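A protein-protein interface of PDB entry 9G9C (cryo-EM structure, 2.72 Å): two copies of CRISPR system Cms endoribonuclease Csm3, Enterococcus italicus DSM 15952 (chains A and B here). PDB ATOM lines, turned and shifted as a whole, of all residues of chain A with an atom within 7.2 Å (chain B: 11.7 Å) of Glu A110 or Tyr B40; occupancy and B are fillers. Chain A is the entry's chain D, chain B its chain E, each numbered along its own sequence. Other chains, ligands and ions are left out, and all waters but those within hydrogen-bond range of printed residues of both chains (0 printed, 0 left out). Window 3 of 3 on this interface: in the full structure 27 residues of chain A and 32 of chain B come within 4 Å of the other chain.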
ATOM      1  N   SER A 104     -21.864   5.396  22.872  1.00  0.00           N
ATOM      2  CA  SER A 104     -22.083   4.596  21.676  1.00  0.00           C
ATOM      3  C   SER A 104     -22.221   3.115  22.011  1.00  0.00           C
ATOM      4  O   SER A 104     -21.733   2.626  23.033  1.00  0.00           O
ATOM      5  CB  SER A 104     -20.941   4.793  20.682  1.00  0.00           C
ATOM      6  OG  SER A 104     -19.700   4.443  21.260  1.00  0.00           O
ATOM      7  N   LYS A 105     -22.908   2.399  21.119  1.00  0.00           N
ATOM      8  CA  LYS A 105     -23.049   0.955  21.267  1.00  0.00           C
ATOM      9  C   LYS A 105     -21.700   0.258  21.148  1.00  0.00           C
ATOM     10  O   LYS A 105     -21.424  -0.704  21.874  1.00  0.00           O
ATOM     11  CB  LYS A 105     -24.025   0.416  20.222  1.00  0.00           C
ATOM     12  CG  LYS A 105     -24.694  -0.891  20.605  1.00  0.00           C
ATOM     13  CD  LYS A 105     -25.944  -0.640  21.431  1.00  0.00           C
ATOM     14  CE  LYS A 105     -27.073  -0.095  20.571  1.00  0.00           C
ATOM     15  NZ  LYS A 105     -28.077   0.655  21.375  1.00  0.00           N
ATOM     16  N   ALA A 106     -20.850   0.725  20.229  1.00  0.00           N
ATOM     17  CA  ALA A 106     -19.529   0.127  20.067  1.00  0.00           C
ATOM     18  C   ALA A 106     -18.688   0.291  21.325  1.00  0.00           C
ATOM     19  O   ALA A 106     -17.984  -0.638  21.737  1.00  0.00           O
ATOM     20  CB  ALA A 106     -18.818   0.744  18.862  1.00  0.00           C
ATOM     21  N   SER A 107     -18.743   1.469  21.949  1.00  0.00           N
ATOM     22  CA  SER A 107     -18.031   1.668  23.205  1.00  0.00           C
ATOM     23  C   SER A 107     -18.604   0.782  24.303  1.00  0.00           C
ATOM     24  O   SER A 107     -17.862   0.278  25.155  1.00  0.00           O
ATOM     25  CB  SER A 107     -18.085   3.139  23.615  1.00  0.00           C
ATOM     26  OG  SER A 107     -17.303   3.376  24.769  1.00  0.00           O
ATOM     27  N   GLN A 108     -19.924   0.578  24.299  1.00  0.00           N
ATOM     28  CA  GLN A 108     -20.533  -0.329  25.265  1.00  0.00           C
ATOM     29  C   GLN A 108     -20.017  -1.750  25.087  1.00  0.00           C
ATOM     30  O   GLN A 108     -19.717  -2.434  26.069  1.00  0.00           O
ATOM     31  CB  GLN A 108     -22.055  -0.303  25.136  1.00  0.00           C
ATOM     32  CG  GLN A 108     -22.706   0.983  25.593  1.00  0.00           C
ATOM     33  CD  GLN A 108     -24.216   0.890  25.597  1.00  0.00           C
ATOM     34  OE1 GLN A 108     -24.889   1.490  24.759  1.00  0.00           O
ATOM     35  NE2 GLN A 108     -24.758   0.133  26.543  1.00  0.00           N
ATOM     36  N   GLU A 109     -19.971  -2.214  23.840  1.00  0.00           N
ATOM     37  CA  GLU A 109     -19.480  -3.589  23.571  1.00  0.00           C
ATOM     38  C   GLU A 109     -18.036  -3.703  24.074  1.00  0.00           C
ATOM     39  O   GLU A 109     -17.764  -4.618  24.869  1.00  0.00           O
ATOM     40  CB  GLU A 109     -19.571  -3.926  22.085  1.00  0.00           C
ATOM     41  CG  GLU A 109     -20.972  -3.751  21.509  1.00  0.00           C
ATOM     42  CD  GLU A 109     -22.092  -4.261  22.397  1.00  0.00           C
ATOM     43  OE1 GLU A 109     -22.132  -5.480  22.665  1.00  0.00           O
ATOM     44  OE2 GLU A 109     -22.922  -3.432  22.827  1.00  0.00           O
ATOM     45  N   GLU A 110     -17.157  -2.792  23.651  1.00  0.00           N
ATOM     46  CA  GLU A 110     -15.726  -2.910  24.024  1.00  0.00           C
ATOM     47  C   GLU A 110     -15.546  -2.810  25.541  1.00  0.00           C
ATOM     48  O   GLU A 110     -14.719  -3.559  26.066  1.00  0.00           O
ATOM     49  CB  GLU A 110     -14.917  -1.749  23.454  1.00  0.00           C
ATOM     50  CG  GLU A 110     -14.929  -1.663  21.933  1.00  0.00           C
ATOM     51  CD  GLU A 110     -14.439  -0.300  21.482  1.00  0.00           C
ATOM     52  OE1 GLU A 110     -13.311   0.069  21.869  1.00  0.00           O
ATOM     53  OE2 GLU A 110     -15.181   0.390  20.750  1.00  0.00           O
ATOM     54  N   PHE A 111     -16.308  -1.950  26.211  1.00  0.00           N
ATOM     55  CA  PHE A 111     -16.141  -1.776  27.677  1.00  0.00           C
ATOM     56  C   PHE A 111     -16.760  -2.979  28.389  1.00  0.00           C
ATOM     57  O   PHE A 111     -16.275  -3.361  29.466  1.00  0.00           O
ATOM     58  CB  PHE A 111     -16.766  -0.481  28.203  1.00  0.00           C
ATOM     59  CG  PHE A 111     -15.971   0.802  28.005  1.00  0.00           C
ATOM     60  CD1 PHE A 111     -15.201   1.008  26.868  1.00  0.00           C
ATOM     61  CD2 PHE A 111     -15.991   1.798  28.972  1.00  0.00           C
ATOM     62  CE1 PHE A 111     -14.486   2.183  26.701  1.00  0.00           C
ATOM     63  CE2 PHE A 111     -15.272   2.968  28.801  1.00  0.00           C
ATOM     64  CZ  PHE A 111     -14.517   3.156  27.669  1.00  0.00           C
ATOM     65  N   ASP A 112     -17.804  -3.571  27.805  1.00  0.00           N
ATOM     66  CA  ASP A 112     -18.412  -4.780  28.424  1.00  0.00           C
ATOM     67  C   ASP A 112     -17.381  -5.903  28.367  1.00  0.00           C
ATOM     68  O   ASP A 112     -17.256  -6.634  29.368  1.00  0.00           O
ATOM     69  CB  ASP A 112     -19.728  -5.155  27.764  1.00  0.00           C
ATOM     70  CG  ASP A 112     -20.917  -4.305  28.186  1.00  0.00           C
ATOM     71  OD1 ASP A 112     -20.733  -3.451  29.078  1.00  0.00           O
ATOM     72  OD2 ASP A 112     -22.006  -4.489  27.607  1.00  0.00           O
ATOM     73  N   LYS A 113     -16.669  -6.039  27.245  1.00  0.00           N
ATOM     74  CA  LYS A 113     -15.549  -7.009  27.231  1.00  0.00           C
ATOM     75  C   LYS A 113     -14.497  -6.426  28.180  1.00  0.00           C
ATOM     76  O   LYS A 113     -14.289  -5.206  28.119  1.00  0.00           O
ATOM     77  CB  LYS A 113     -15.042  -7.183  25.799  1.00  0.00           C
ATOM     78  CG  LYS A 113     -16.142  -7.513  24.803  1.00  0.00           C
ATOM     79  CD  LYS A 113     -15.872  -6.994  23.397  1.00  0.00           C
ATOM     80  CE  LYS A 113     -17.076  -7.117  22.518  1.00  0.00           C
ATOM     81  NZ  LYS A 113     -16.880  -6.436  21.236  1.00  0.00           N
ATOM     82  N   LYS A 114     -13.909  -7.242  29.048  1.00  0.00           N
ATOM     83  CA  LYS A 114     -12.891  -6.786  30.038  1.00  0.00           C
ATOM     84  C   LYS A 114     -13.639  -6.158  31.222  1.00  0.00           C
ATOM     85  O   LYS A 114     -12.960  -5.655  32.141  1.00  0.00           O
ATOM     86  CB  LYS A 114     -11.831  -5.829  29.476  1.00  0.00           C
ATOM     87  CG  LYS A 114     -10.954  -6.426  28.386  1.00  0.00           C
ATOM     88  CD  LYS A 114     -10.159  -5.375  27.624  1.00  0.00           C
ATOM     89  CE  LYS A 114      -9.145  -5.982  26.709  1.00  0.00           C
ATOM     90  NZ  LYS A 114      -8.243  -4.963  26.165  1.00  0.00           N
ATOM     91  N   ASP A 115     -14.973  -6.150  31.178  1.00  0.00           N
ATOM     92  CA  ASP A 115     -15.785  -5.676  32.332  1.00  0.00           C
ATOM     93  C   ASP A 115     -15.350  -4.261  32.723  1.00  0.00           C
ATOM     94  O   ASP A 115     -15.275  -3.984  33.939  1.00  0.00           O
ATOM     95  CB  ASP A 115     -15.731  -6.672  33.480  1.00  0.00           C
ATOM     96  CG  ASP A 115     -16.134  -8.094  33.120  1.00  0.00           C
ATOM     97  OD1 ASP A 115     -16.469  -8.328  31.940  1.00  0.00           O
ATOM     98  OD2 ASP A 115     -16.110  -8.955  34.023  1.00  0.00           O
ATOM     99  N   LEU A 116     -15.126  -3.381  31.747  1.00  0.00           N
ATOM    100  CA  LEU A 116     -14.667  -2.002  32.054  1.00  0.00           C
ATOM    101  C   LEU A 116     -15.878  -1.118  32.380  1.00  0.00           C
ATOM    102  O   LEU A 116     -16.816  -1.081  31.561  1.00  0.00           O
ATOM    103  CB  LEU A 116     -13.865  -1.431  30.886  1.00  0.00           C
ATOM    104  CG  LEU A 116     -13.256  -0.044  31.114  1.00  0.00           C
ATOM    105  CD1 LEU A 116     -12.332  -0.062  32.316  1.00  0.00           C
ATOM    106  CD2 LEU A 116     -12.511   0.412  29.879  1.00  0.00           C
ATOM    107  N   TYR A 118     -18.124   2.151  32.490  1.00  0.00           N
ATOM    108  CA  TYR A 118     -18.249   3.278  31.524  1.00  0.00           C
ATOM    109  C   TYR A 118     -17.636   4.538  32.125  1.00  0.00           C
ATOM    110  O   TYR A 118     -17.008   5.313  31.378  1.00  0.00           O
ATOM    111  CB  TYR A 118     -19.723   3.426  31.143  1.00  0.00           C
ATOM    112  CG  TYR A 118     -20.312   2.209  30.447  1.00  0.00           C
ATOM    113  CD1 TYR A 118     -19.523   1.371  29.669  1.00  0.00           C
ATOM    114  CD2 TYR A 118     -21.660   1.898  30.568  1.00  0.00           C
ATOM    115  CE1 TYR A 118     -20.054   0.263  29.033  1.00  0.00           C
ATOM    116  CE2 TYR A 118     -22.202   0.791  29.939  1.00  0.00           C
ATOM    117  CZ  TYR A 118     -21.398  -0.027  29.168  1.00  0.00           C
ATOM    118  OH  TYR A 118     -21.937  -1.116  28.549  1.00  0.00           O
ATOM    119  N   THR A 143     -14.837   7.146  31.097  1.00  0.00           N
ATOM    120  CA  THR A 143     -13.505   6.530  30.899  1.00  0.00           C
ATOM    121  C   THR A 143     -12.928   6.879  29.547  1.00  0.00           C
ATOM    122  O   THR A 143     -13.695   6.917  28.569  1.00  0.00           O
ATOM    123  CB  THR A 143     -13.629   5.019  31.089  1.00  0.00           C
ATOM    124  OG1 THR A 143     -14.173   4.850  32.393  1.00  0.00           O
ATOM    125  CG2 THR A 143     -12.300   4.294  30.989  1.00  0.00           C
ATOM    126  N   ARG A 144     -11.614   7.110  29.486  1.00  0.00           N
ATOM    127  CA  ARG A 144     -10.938   7.344  28.186  1.00  0.00           C
ATOM    128  C   ARG A 144     -11.213   6.139  27.284  1.00  0.00           C
ATOM    129  O   ARG A 144     -11.324   5.016  27.809  1.00  0.00           O
ATOM    130  CB  ARG A 144      -9.439   7.578  28.396  1.00  0.00           C
ATOM    131  CG  ARG A 144      -8.667   7.947  27.140  1.00  0.00           C
ATOM    132  CD  ARG A 144      -7.181   7.652  27.265  1.00  0.00           C
ATOM    133  NE  ARG A 144      -6.853   6.247  27.536  1.00  0.00           N
ATOM    134  CZ  ARG A 144      -7.070   5.202  26.742  1.00  0.00           C
ATOM    135  NH1 ARG A 144      -7.750   5.330  25.616  1.00  0.00           N
ATOM    136  NH2 ARG A 144      -6.591   4.018  27.078  1.00  0.00           N
ATOM    137  N   GLY A 145     -11.255   6.351  25.976  1.00  0.00           N
ATOM    138  CA  GLY A 145     -11.621   5.317  25.035  1.00  0.00           C
ATOM    139  C   GLY A 145     -13.107   5.189  24.803  1.00  0.00           C
ATOM    140  O   GLY A 145     -13.530   4.276  24.084  1.00  0.00           O
ATOM    141  N   ALA A 146     -13.910   6.069  25.393  1.00  0.00           N
ATOM    142  CA  ALA A 146     -15.349   6.067  25.199  1.00  0.00           C
ATOM    143  C   ALA A 146     -15.708   6.889  23.970  1.00  0.00           C
ATOM    144  O   ALA A 146     -15.071   7.904  23.679  1.00  0.00           O
ATOM    145  CB  ALA A 146     -16.060   6.628  26.430  1.00  0.00           C
ATOM    146  N   SER A 147     -16.732   6.440  23.252  1.00  0.00           N
ATOM    147  CA  SER A 147     -17.188   7.092  22.035  1.00  0.00           C
ATOM    148  C   SER A 147     -18.649   7.478  22.191  1.00  0.00           C
ATOM    149  O   SER A 147     -19.450   6.695  22.709  1.00  0.00           O
ATOM    150  CB  SER A 147     -17.006   6.179  20.821  1.00  0.00           C
ATOM    151  OG  SER A 147     -15.636   5.915  20.583  1.00  0.00           O
ATOM    152  N   VAL B  35      -1.387   3.071  42.716  1.00  0.00           N
ATOM    153  CA  VAL B  35      -1.210   4.283  41.924  1.00  0.00           C
ATOM    154  C   VAL B  35      -2.418   4.456  41.018  1.00  0.00           C
ATOM    155  O   VAL B  35      -3.099   3.487  40.660  1.00  0.00           O
ATOM    156  CB  VAL B  35       0.091   4.241  41.094  1.00  0.00           C
ATOM    157  CG1 VAL B  35       1.302   4.273  41.999  1.00  0.00           C
ATOM    158  CG2 VAL B  35       0.114   3.015  40.198  1.00  0.00           C
ATOM    159  N   VAL B  36      -2.672   5.707  40.629  1.00  0.00           N
ATOM    160  CA  VAL B  36      -3.774   5.976  39.660  1.00  0.00           C
ATOM    161  C   VAL B  36      -3.356   5.371  38.312  1.00  0.00           C
ATOM    162  O   VAL B  36      -2.207   5.598  37.882  1.00  0.00           O
ATOM    163  CB  VAL B  36      -4.103   7.477  39.533  1.00  0.00           C
ATOM    164  CG1 VAL B  36      -2.870   8.330  39.264  1.00  0.00           C
ATOM    165  CG2 VAL B  36      -5.185   7.746  38.495  1.00  0.00           C
ATOM    166  N   ARG B  37      -4.243   4.601  37.693  1.00  0.00           N
ATOM    167  CA  ARG B  37      -3.931   3.957  36.398  1.00  0.00           C
ATOM    168  C   ARG B  37      -5.064   4.285  35.422  1.00  0.00           C
ATOM    169  O   ARG B  37      -6.214   4.388  35.886  1.00  0.00           O
ATOM    170  CB  ARG B  37      -3.786   2.445  36.606  1.00  0.00           C
ATOM    171  CG  ARG B  37      -2.704   2.083  37.612  1.00  0.00           C
ATOM    172  CD  ARG B  37      -2.606   0.595  37.887  1.00  0.00           C
ATOM    173  NE  ARG B  37      -1.978  -0.118  36.770  1.00  0.00           N
ATOM    174  CZ  ARG B  37      -0.858  -0.817  36.866  1.00  0.00           C
ATOM    175  NH1 ARG B  37      -0.334  -1.061  38.052  1.00  0.00           N
ATOM    176  NH2 ARG B  37      -0.269  -1.276  35.776  1.00  0.00           N
ATOM    177  N   ASP B  38      -4.761   4.460  34.132  1.00  0.00           N
ATOM    178  CA  ASP B  38      -5.875   4.661  33.173  1.00  0.00           C
ATOM    179  C   ASP B  38      -6.704   3.377  33.197  1.00  0.00           C
ATOM    180  O   ASP B  38      -6.110   2.293  33.090  1.00  0.00           O
ATOM    181  CB  ASP B  38      -5.340   4.961  31.785  1.00  0.00           C
ATOM    182  CG  ASP B  38      -6.339   4.860  30.642  1.00  0.00           C
ATOM    183  OD1 ASP B  38      -7.311   5.642  30.638  1.00  0.00           O
ATOM    184  OD2 ASP B  38      -6.133   4.002  29.763  1.00  0.00           O
ATOM    185  N   PRO B  39      -8.046   3.446  33.290  1.00  0.00           N
ATOM    186  CA  PRO B  39      -8.850   2.238  33.381  1.00  0.00           C
ATOM    187  C   PRO B  39      -8.769   1.356  32.152  1.00  0.00           C
ATOM    188  O   PRO B  39      -8.681   0.126  32.295  1.00  0.00           O
ATOM    189  CB  PRO B  39     -10.254   2.820  33.590  1.00  0.00           C
ATOM    190  CG  PRO B  39     -10.002   4.183  34.181  1.00  0.00           C
ATOM    191  CD  PRO B  39      -8.813   4.673  33.387  1.00  0.00           C
ATOM    192  N   TYR B  40      -8.779   1.963  30.967  1.00  0.00           N
ATOM    193  CA  TYR B  40      -8.809   1.181  29.704  1.00  0.00           C
ATOM    194  C   TYR B  40      -7.509   0.417  29.530  1.00  0.00           C
ATOM    195  O   TYR B  40      -7.552  -0.812  29.323  1.00  0.00           O
ATOM    196  CB  TYR B  40      -9.034   2.217  28.602  1.00  0.00           C
ATOM    197  CG  TYR B  40      -9.539   1.668  27.276  1.00  0.00           C
ATOM    198  CD1 TYR B  40      -8.658   1.228  26.297  1.00  0.00           C
ATOM    199  CD2 TYR B  40     -10.898   1.598  27.004  1.00  0.00           C
ATOM    200  CE1 TYR B  40      -9.116   0.730  25.089  1.00  0.00           C
ATOM    201  CE2 TYR B  40     -11.368   1.100  25.801  1.00  0.00           C
ATOM    202  CZ  TYR B  40     -10.474   0.666  24.841  1.00  0.00           C
ATOM    203  OH  TYR B  40     -10.937   0.177  23.654  1.00  0.00           O
ATOM    204  N   SER B  41      -6.380   1.119  29.609  1.00  0.00           N
ATOM    205  CA  SER B  41      -5.051   0.492  29.388  1.00  0.00           C
ATOM    206  C   SER B  41      -4.530  -0.175  30.666  1.00  0.00           C
ATOM    207  O   SER B  41      -3.569  -0.952  30.550  1.00  0.00           O
ATOM    208  CB  SER B  41      -4.059   1.495  28.876  1.00  0.00           C
ATOM    209  OG  SER B  41      -3.775   2.473  29.864  1.00  0.00           O
ATOM    210  N   ARG B  42      -5.169   0.068  31.810  1.00  0.00           N
ATOM    211  CA  ARG B  42      -4.669  -0.463  33.107  1.00  0.00           C
ATOM    212  C   ARG B  42      -3.234   0.043  33.326  1.00  0.00           C
ATOM    213  O   ARG B  42      -2.588  -0.434  34.279  1.00  0.00           O
ATOM    214  CB  ARG B  42      -4.815  -1.988  33.154  1.00  0.00           C
ATOM    215  CG  ARG B  42      -6.177  -2.480  32.686  1.00  0.00           C
ATOM    216  CD  ARG B  42      -6.460  -3.891  33.162  1.00  0.00           C
ATOM    217  NE  ARG B  42      -6.592  -3.942  34.621  1.00  0.00           N
ATOM    218  CZ  ARG B  42      -6.839  -5.043  35.317  1.00  0.00           C
ATOM    219  NH1 ARG B  42      -6.875  -6.214  34.710  1.00  0.00           N
ATOM    220  NH2 ARG B  42      -7.036  -4.968  36.621  1.00  0.00           N
ATOM    221  N   LEU B  43      -2.772   0.969  32.488  1.00  0.00           N
ATOM    222  CA  LEU B  43      -1.394   1.509  32.611  1.00  0.00           C
ATOM    223  C   LEU B  43      -1.434   2.742  33.515  1.00  0.00           C
ATOM    224  O   LEU B  43      -2.387   3.530  33.395  1.00  0.00           O
ATOM    225  CB  LEU B  43      -0.824   1.865  31.238  1.00  0.00           C
ATOM    226  CG  LEU B  43       0.160   0.872  30.615  1.00  0.00           C
ATOM    227  CD1 LEU B  43      -0.473  -0.484  30.402  1.00  0.00           C
ATOM    228  CD2 LEU B  43       0.646   1.426  29.292  1.00  0.00           C
ATOM    229  N   PRO B  44      -0.436   2.953  34.396  1.00  0.00           N
ATOM    230  CA  PRO B  44      -0.399   4.158  35.210  1.00  0.00           C
ATOM    231  C   PRO B  44      -0.481   5.452  34.395  1.00  0.00           C
ATOM    232  O   PRO B  44      -0.044   5.467  33.229  1.00  0.00           O
ATOM    233  CB  PRO B  44       0.942   4.007  35.947  1.00  0.00           C
ATOM    234  CG  PRO B  44       1.720   3.000  35.137  1.00  0.00           C
ATOM    235  CD  PRO B  44       0.665   2.042  34.634  1.00  0.00           C
ATOM    236  N   ILE B  45      -1.042   6.513  34.985  1.00  0.00           N
ATOM    237  CA  ILE B  45      -1.106   7.827  34.297  1.00  0.00           C
ATOM    238  C   ILE B  45      -0.693   8.922  35.278  1.00  0.00           C
ATOM    239  O   ILE B  45      -0.858   8.717  36.495  1.00  0.00           O
ATOM    240  CB  ILE B  45      -2.529   8.111  33.787  1.00  0.00           C
ATOM    241  CG1 ILE B  45      -3.577   7.807  34.853  1.00  0.00           C
ATOM    242  CG2 ILE B  45      -2.807   7.359  32.486  1.00  0.00           C
ATOM    243  CD1 ILE B  45      -4.968   8.300  34.503  1.00  0.00           C
ATOM    244  N   ASP B 100      -3.535  14.913  30.983  1.00  0.00           N
ATOM    245  CA  ASP B 100      -3.011  13.738  31.716  1.00  0.00           C
ATOM    246  C   ASP B 100      -1.858  13.142  30.915  1.00  0.00           C
ATOM    247  O   ASP B 100      -2.023  12.973  29.698  1.00  0.00           O
ATOM    248  CB  ASP B 100      -4.113  12.717  31.935  1.00  0.00           C
ATOM    249  CG  ASP B 100      -5.285  13.189  32.784  1.00  0.00           C
ATOM    250  OD1 ASP B 100      -5.212  14.319  33.306  1.00  0.00           O
ATOM    251  OD2 ASP B 100      -6.266  12.427  32.903  1.00  0.00           O
ATOM    252  N   PHE B 102       0.452  10.113  29.710  1.00  0.00           N
ATOM    253  CA  PHE B 102       0.094   8.687  29.511  1.00  0.00           C
ATOM    254  C   PHE B 102       1.387   7.911  29.342  1.00  0.00           C
ATOM    255  O   PHE B 102       2.354   8.469  28.789  1.00  0.00           O
ATOM    256  CB  PHE B 102      -0.855   8.505  28.323  1.00  0.00           C
ATOM    257  CG  PHE B 102      -2.189   9.229  28.450  1.00  0.00           C
ATOM    258  CD1 PHE B 102      -3.220   8.691  29.210  1.00  0.00           C
ATOM    259  CD2 PHE B 102      -2.423  10.424  27.781  1.00  0.00           C
ATOM    260  CE1 PHE B 102      -4.435   9.346  29.324  1.00  0.00           C
ATOM    261  CE2 PHE B 102      -3.644  11.071  27.892  1.00  0.00           C
ATOM    262  CZ  PHE B 102      -4.644  10.533  28.665  1.00  0.00           C
ATOM    263  N   PHE B 103       1.417   6.664  29.818  1.00  0.00           N
ATOM    264  CA  PHE B 103       2.689   5.905  29.784  1.00  0.00           C
ATOM    265  C   PHE B 103       3.100   5.776  28.338  1.00  0.00           C
ATOM    266  O   PHE B 103       2.254   5.422  27.491  1.00  0.00           O
ATOM    267  CB  PHE B 103       2.291   4.574  30.421  1.00  0.00           C
ATOM    268  CG  PHE B 103       3.396   3.633  30.875  1.00  0.00           C
ATOM    269  CD1 PHE B 103       3.988   2.742  29.988  1.00  0.00           C
ATOM    270  CD2 PHE B 103       3.823   3.625  32.195  1.00  0.00           C
ATOM    271  CE1 PHE B 103       4.983   1.878  30.410  1.00  0.00           C
ATOM    272  CE2 PHE B 103       4.813   2.754  32.612  1.00  0.00           C
ATOM    273  CZ  PHE B 103       5.396   1.890  31.718  1.00  0.00           C
ATOM    274  N   LYS B 105       4.415   4.463  24.796  1.00  0.00           N
ATOM    275  CA  LYS B 105       4.453   3.132  24.138  1.00  0.00           C
ATOM    276  C   LYS B 105       5.914   2.663  24.103  1.00  0.00           C
ATOM    277  O   LYS B 105       6.160   1.466  24.310  1.00  0.00           O
ATOM    278  CB  LYS B 105       3.856   3.177  22.728  1.00  0.00           C
ATOM    279  CG  LYS B 105       4.027   1.904  21.908  1.00  0.00           C
ATOM    280  CD  LYS B 105       3.393   0.668  22.536  1.00  0.00           C
ATOM    281  CE  LYS B 105       1.901   0.754  22.574  1.00  0.00           C
ATOM    282  NZ  LYS B 105       1.306  -0.464  23.129  1.00  0.00           N
ATOM    283  N   GLN B 108       6.734   1.387  27.299  1.00  0.00           N
ATOM    284  CA  GLN B 108       5.985   0.114  27.397  1.00  0.00           C
ATOM    285  C   GLN B 108       6.763  -0.964  26.636  1.00  0.00           C
ATOM    286  O   GLN B 108       6.969  -2.048  27.211  1.00  0.00           O
ATOM    287  CB  GLN B 108       4.582   0.307  26.826  1.00  0.00           C
ATOM    288  CG  GLN B 108       3.722  -0.949  26.825  1.00  0.00           C
ATOM    289  CD  GLN B 108       2.278  -0.666  26.483  1.00  0.00           C
ATOM    290  OE1 GLN B 108       1.902   0.470  26.171  1.00  0.00           O
ATOM    291  NE2 GLN B 108       1.453  -1.700  26.531  1.00  0.00           N
ATOM    292  N   TYR B 118       5.448  -2.598  34.890  1.00  0.00           N
ATOM    293  CA  TYR B 118       5.360  -1.142  34.855  1.00  0.00           C
ATOM    294  C   TYR B 118       5.452  -0.550  36.254  1.00  0.00           C
ATOM    295  O   TYR B 118       6.071   0.501  36.453  1.00  0.00           O
ATOM    296  CB  TYR B 118       4.060  -0.712  34.178  1.00  0.00           C
ATOM    297  CG  TYR B 118       3.849  -1.332  32.817  1.00  0.00           C
ATOM    298  CD1 TYR B 118       4.919  -1.566  31.963  1.00  0.00           C
ATOM    299  CD2 TYR B 118       2.582  -1.699  32.392  1.00  0.00           C
ATOM    300  CE1 TYR B 118       4.729  -2.138  30.724  1.00  0.00           C
ATOM    301  CE2 TYR B 118       2.384  -2.271  31.155  1.00  0.00           C
ATOM    302  CZ  TYR B 118       3.460  -2.488  30.326  1.00  0.00           C
ATOM    303  OH  TYR B 118       3.263  -3.060  29.092  1.00  0.00           O
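Of the 19 printed residues of chain A, 5 touch a printed residue of chain B. Among the printed residues, 9 pairs touch across the chains. Among the printed residues, Asp or Glu carboxylates within 4 Å of a Lys or Arg side-chain nitrogen of the other chain: Arg A144 with Asp B38 (2.7 Å).
OD2 of Asp B38 lies within salt-bridge range of NH2 of Arg A144. OH of Tyr B40 sits at hydrogen-bond distance from OE1 of Glu A110, at 3.0 Å.
No residue of chain B comes within 4 Å of Ala A106. No residue of chain B comes within 4 Å of Ser A107. Of chain B, only Tyr B40 comes within 4 Å of Glu A110. Phe A111 touches one residue of chain B. No residue of chain B comes within 4 Å of Asp A112. No residue of chain B comes within 4 Å of Lys A114. Of chain B, only Pro B39 (3.7 Å) and Tyr B40 (3.5 Å) come within 4 Å of Leu A116. Of the printed residues of chain B, Thr A143 touches Pro B39. Of chain B, only Asp B38, Tyr B40, Ser B41 and Phe B102 come within 4 Å of Arg A144. No residue of chain B comes within 4 Å of Gly A145. Of the printed residues of chain A, Asp B38 touches Arg A144 (2.7 Å). Printed residues of chain A within 4 Å of Pro B39: Leu A116 and Thr A143. Of the printed residues of chain A, Ser B41 touches Arg A144 (3.9 Å). Printed residues of chain A within 4 Å of Phe B102: Arg A144. The nearest residue of chain B that does not touch Glu A110 is Pro B39 (9.4 Å).
Among the printed residues, pairs that only touch across the chains: Phe A111 with Tyr B40 (3.4 Å), Leu A116 with Pro B39 (3.7 Å), Leu A116 with Tyr B40 (3.5 Å), Thr A143 with Pro B39 (3.6 Å), Arg A144 with Tyr B40 (3.4 Å), Arg A144 with Ser B41 (3.9 Å) and Arg A144 with Phe B102 (3.8 Å).
The side-chain carboxylate (OD2) of Asp B38 lies within hydrogen-bond range of the side-chain hydroxyl (OG) of Ser B41. The backbone NH (N) of Asp B38 sits at hydrogen-bond distance from the backbone carbonyl oxygen (O) of Leu B43, at 2.7 Å. OG of Ser B41 lies close to N of Leu B43. N of Leu A116 lies within hydrogen-bond range of O of Phe A111, at 2.6 Å. O of Tyr A118 is in hydrogen-bond range of N of Thr A143.
Positions printed for both chains: 105, 108 and 118. Of the 9 pairs that touch across the chains among the printed residues, none has its exchanged pair printed and touching as well.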
